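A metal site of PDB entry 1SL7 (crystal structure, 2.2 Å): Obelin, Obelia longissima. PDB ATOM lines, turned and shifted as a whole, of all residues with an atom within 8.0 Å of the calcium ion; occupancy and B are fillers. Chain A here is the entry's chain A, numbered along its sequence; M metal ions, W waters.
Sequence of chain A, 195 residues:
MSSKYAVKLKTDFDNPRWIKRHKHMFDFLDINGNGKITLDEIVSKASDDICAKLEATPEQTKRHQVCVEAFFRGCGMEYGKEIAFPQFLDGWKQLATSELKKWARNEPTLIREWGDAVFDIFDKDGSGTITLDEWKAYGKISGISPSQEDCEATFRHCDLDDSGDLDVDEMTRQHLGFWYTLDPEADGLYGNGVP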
ATOM      1  N   PHE A  26      -6.562 -35.389  12.917  1.00  0.00           N
ATOM      2  CA  PHE A  26      -5.944 -34.106  13.295  1.00  0.00           C
ATOM      3  C   PHE A  26      -4.573 -34.270  13.924  1.00  0.00           C
ATOM      4  O   PHE A  26      -3.614 -33.603  13.505  1.00  0.00           O
ATOM      5  CB  PHE A  26      -6.903 -33.335  14.240  1.00  0.00           C
ATOM      6  CG  PHE A  26      -6.413 -31.932  14.664  1.00  0.00           C
ATOM      7  CD1 PHE A  26      -6.987 -30.774  14.094  1.00  0.00           C
ATOM      8  CD2 PHE A  26      -5.457 -31.765  15.679  1.00  0.00           C
ATOM      9  CE1 PHE A  26      -6.587 -29.494  14.485  1.00  0.00           C
ATOM     10  CE2 PHE A  26      -5.055 -30.485  16.086  1.00  0.00           C
ATOM     11  CZ  PHE A  26      -5.616 -29.344  15.480  1.00  0.00           C
ATOM     12  N   ASP A  27      -4.447 -35.146  14.931  1.00  0.00           N
ATOM     13  CA  ASP A  27      -3.151 -35.342  15.606  1.00  0.00           C
ATOM     14  C   ASP A  27      -2.095 -35.987  14.687  1.00  0.00           C
ATOM     15  O   ASP A  27      -0.906 -35.718  14.829  1.00  0.00           O
ATOM     16  CB  ASP A  27      -3.308 -36.140  16.925  1.00  0.00           C
ATOM     17  CG  ASP A  27      -4.076 -35.350  18.012  1.00  0.00           C
ATOM     18  OD1 ASP A  27      -4.123 -34.095  17.999  1.00  0.00           O
ATOM     19  OD2 ASP A  27      -4.686 -35.908  18.942  1.00  0.00           O
ATOM     20  N   LEU A  29      -2.006 -35.477  11.271  1.00  0.00           N
ATOM     21  CA  LEU A  29      -1.597 -34.382  10.357  1.00  0.00           C
ATOM     22  C   LEU A  29      -0.711 -33.291  11.027  1.00  0.00           C
ATOM     23  O   LEU A  29       0.061 -32.615  10.347  1.00  0.00           O
ATOM     24  CB  LEU A  29      -2.828 -33.727   9.691  1.00  0.00           C
ATOM     25  CG  LEU A  29      -3.774 -34.609   8.829  1.00  0.00           C
ATOM     26  CD1 LEU A  29      -5.029 -33.821   8.422  1.00  0.00           C
ATOM     27  CD2 LEU A  29      -3.067 -35.124   7.601  1.00  0.00           C
ATOM     28  N   ASP A  30      -0.818 -33.168  12.357  1.00  0.00           N
ATOM     29  CA  ASP A  30      -0.042 -32.190  13.154  1.00  0.00           C
ATOM     30  C   ASP A  30       1.447 -32.620  13.310  1.00  0.00           C
ATOM     31  O   ASP A  30       1.842 -33.159  14.357  1.00  0.00           O
ATOM     32  CB  ASP A  30      -0.744 -31.996  14.508  1.00  0.00           C
ATOM     33  CG  ASP A  30      -0.006 -31.066  15.485  1.00  0.00           C
ATOM     34  OD1 ASP A  30       0.828 -30.187  15.086  1.00  0.00           O
ATOM     35  OD2 ASP A  30      -0.237 -31.142  16.707  1.00  0.00           O
ATOM     36  N   ILE A  31       2.261 -32.373  12.286  1.00  0.00           N
ATOM     37  CA  ILE A  31       3.666 -32.838  12.255  1.00  0.00           C
ATOM     38  C   ILE A  31       4.509 -32.492  13.498  1.00  0.00           C
ATOM     39  O   ILE A  31       5.104 -33.384  14.109  1.00  0.00           O
ATOM     40  CB  ILE A  31       4.377 -32.363  10.957  1.00  0.00           C
ATOM     41  CG1 ILE A  31       3.678 -32.916   9.713  1.00  0.00           C
ATOM     42  CG2 ILE A  31       5.894 -32.742  10.968  1.00  0.00           C
ATOM     43  CD1 ILE A  31       4.167 -32.302   8.385  1.00  0.00           C
ATOM     44  N   ASN A  32       4.552 -31.206  13.880  1.00  0.00           N
ATOM     45  CA  ASN A  32       5.388 -30.762  15.019  1.00  0.00           C
ATOM     46  C   ASN A  32       4.765 -30.939  16.424  1.00  0.00           C
ATOM     47  O   ASN A  32       5.377 -30.532  17.425  1.00  0.00           O
ATOM     48  CB  ASN A  32       5.895 -29.325  14.810  1.00  0.00           C
ATOM     49  CG  ASN A  32       4.811 -28.266  15.011  1.00  0.00           C
ATOM     50  OD1 ASN A  32       3.647 -28.571  15.321  1.00  0.00           O
ATOM     51  ND2 ASN A  32       5.188 -27.012  14.840  1.00  0.00           N
ATOM     52  N   GLY A  33       3.583 -31.539  16.494  1.00  0.00           N
ATOM     53  CA  GLY A  33       2.940 -31.859  17.770  1.00  0.00           C
ATOM     54  C   GLY A  33       2.513 -30.710  18.684  1.00  0.00           C
ATOM     55  O   GLY A  33       2.212 -30.940  19.853  1.00  0.00           O
ATOM     56  N   ASN A  34       2.466 -29.484  18.175  1.00  0.00           N
ATOM     57  CA  ASN A  34       2.073 -28.337  19.020  1.00  0.00           C
ATOM     58  C   ASN A  34       0.552 -28.146  19.292  1.00  0.00           C
ATOM     59  O   ASN A  34       0.141 -27.160  19.885  1.00  0.00           O
ATOM     60  CB  ASN A  34       2.716 -27.033  18.520  1.00  0.00           C
ATOM     61  CG  ASN A  34       1.993 -26.430  17.325  1.00  0.00           C
ATOM     62  OD1 ASN A  34       1.250 -27.110  16.608  1.00  0.00           O
ATOM     63  ND2 ASN A  34       2.240 -25.134  17.096  1.00  0.00           N
ATOM     64  N   GLY A  35      -0.279 -29.101  18.857  1.00  0.00           N
ATOM     65  CA  GLY A  35      -1.714 -28.977  19.060  1.00  0.00           C
ATOM     66  C   GLY A  35      -2.480 -28.019  18.152  1.00  0.00           C
ATOM     67  O   GLY A  35      -3.652 -27.739  18.426  1.00  0.00           O
ATOM     68  N   LYS A  36      -1.827 -27.488  17.094  1.00  0.00           N
ATOM     69  CA  LYS A  36      -2.497 -26.702  16.046  1.00  0.00           C
ATOM     70  C   LYS A  36      -2.017 -27.083  14.650  1.00  0.00           C
ATOM     71  O   LYS A  36      -0.847 -27.441  14.493  1.00  0.00           O
ATOM     72  CB  LYS A  36      -2.278 -25.191  16.232  1.00  0.00           C
ATOM     73  CG  LYS A  36      -2.429 -24.691  17.652  1.00  0.00           C
ATOM     74  CD  LYS A  36      -2.629 -23.196  17.686  1.00  0.00           C
ATOM     75  CE  LYS A  36      -2.591 -22.674  19.114  1.00  0.00           C
ATOM     76  NZ  LYS A  36      -3.631 -21.637  19.292  1.00  0.00           N
ATOM     77  N   ILE A  37      -2.896 -27.003  13.639  1.00  0.00           N
ATOM     78  CA  ILE A  37      -2.511 -27.326  12.255  1.00  0.00           C
ATOM     79  C   ILE A  37      -2.552 -26.150  11.280  1.00  0.00           C
ATOM     80  O   ILE A  37      -3.357 -25.223  11.439  1.00  0.00           O
ATOM     81  CB  ILE A  37      -3.314 -28.504  11.639  1.00  0.00           C
ATOM     82  CG1 ILE A  37      -4.813 -28.223  11.656  1.00  0.00           C
ATOM     83  CG2 ILE A  37      -2.932 -29.843  12.272  1.00  0.00           C
ATOM     84  CD1 ILE A  37      -5.585 -29.268  10.883  1.00  0.00           C
ATOM     85  N   THR A  38      -1.684 -26.227  10.270  1.00  0.00           N
ATOM     86  CA  THR A  38      -1.604 -25.282   9.158  1.00  0.00           C
ATOM     87  C   THR A  38      -1.807 -26.024   7.836  1.00  0.00           C
ATOM     88  O   THR A  38      -1.627 -27.249   7.761  1.00  0.00           O
ATOM     89  CB  THR A  38      -0.202 -24.679   9.092  1.00  0.00           C
ATOM     90  OG1 THR A  38       0.756 -25.741   9.101  1.00  0.00           O
ATOM     91  CG2 THR A  38       0.136 -23.848  10.347  1.00  0.00           C
ATOM     92  N   GLU A  41       1.408 -28.157   6.894  1.00  0.00           N
ATOM     93  CA  GLU A  41       1.427 -29.512   7.460  1.00  0.00           C
ATOM     94  C   GLU A  41       0.480 -30.480   6.727  1.00  0.00           C
ATOM     95  O   GLU A  41       0.864 -31.626   6.460  1.00  0.00           O
ATOM     96  CB  GLU A  41       1.106 -29.486   8.979  1.00  0.00           C
ATOM     97  CG  GLU A  41       2.221 -28.907   9.862  1.00  0.00           C
ATOM     98  CD  GLU A  41       1.886 -28.862  11.359  1.00  0.00           C
ATOM     99  OE1 GLU A  41       0.703 -28.656  11.729  1.00  0.00           O
ATOM    100  OE2 GLU A  41       2.815 -29.002  12.194  1.00  0.00           O
ATOM    101  N   GLU A  82      -2.276 -20.978  11.987  1.00  0.00           N
ATOM    102  CA  GLU A  82      -2.427 -22.045  12.982  1.00  0.00           C
ATOM    103  C   GLU A  82      -3.838 -22.103  13.556  1.00  0.00           C
ATOM    104  O   GLU A  82      -4.320 -21.101  14.083  1.00  0.00           O
ATOM    105  CB  GLU A  82      -1.432 -21.877  14.125  1.00  0.00           C
ATOM    106  CG  GLU A  82       0.023 -21.898  13.686  1.00  0.00           C
ATOM    107  CD  GLU A  82       0.937 -22.444  14.744  1.00  0.00           C
ATOM    108  OE1 GLU A  82       1.080 -21.787  15.812  1.00  0.00           O
ATOM    109  OE2 GLU A  82       1.524 -23.519  14.518  1.00  0.00           O
ATOM    110  N   ILE A  83      -4.480 -23.269  13.459  1.00  0.00           N
ATOM    111  CA  ILE A  83      -5.871 -23.482  13.939  1.00  0.00           C
ATOM    112  C   ILE A  83      -5.939 -24.713  14.842  1.00  0.00           C
ATOM    113  O   ILE A  83      -5.405 -25.779  14.478  1.00  0.00           O
ATOM    114  CB  ILE A  83      -6.859 -23.645  12.730  1.00  0.00           C
ATOM    115  CG1 ILE A  83      -6.711 -22.533  11.689  1.00  0.00           C
ATOM    116  CG2 ILE A  83      -8.329 -23.787  13.214  1.00  0.00           C
ATOM    117  CD1 ILE A  83      -7.164 -21.147  12.132  1.00  0.00           C
HETATM  118 CA    CA M   1       1.352 -28.117  14.297  1.00  0.00          CA
HETATM  119  O   HOH W   1       2.034 -25.848  13.489  1.00  0.00           O
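The calcium ion is bound by the side-chain carboxylate (OD1) of Asp 30, the backbone carbonyl oxygen (O) of Lys 36, water W1, the side-chain amide oxygen (OD1) of Asn 34, the side-chain amide oxygen (OD1) of Asn 32, the side-chain carboxylate (OE1) of Glu 41 and the side-chain carboxylate (OE2) of Glu 41.
The calcium ion has seven donor atoms within binding distance.
ND2 of Asn 34 sits at hydrogen-bond distance from OE2 of Glu 82 (3.1 Å).
The side-chain carboxylate of Asp 30 sits at hydrogen-bond distance from the backbone NH of Gly 35 (3.0 Å).
The side-chain hydroxyl (OG1) of Thr 38 sits at hydrogen-bond distance from the backbone NH (N) of Glu 41, at 3.3 Å.
The backbone NH of Ile 31 lies close to the side-chain carboxylate of Glu 41, 3.4 Å away.
The side-chain carboxylate (OD1) of Asp 30 lies close to the backbone NH (N) of Gly 33, at 3.4 Å.
Within 4 Å of the calcium ion: Asp 30, Asn 32, Asn 34, Lys 36 and Glu 41.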
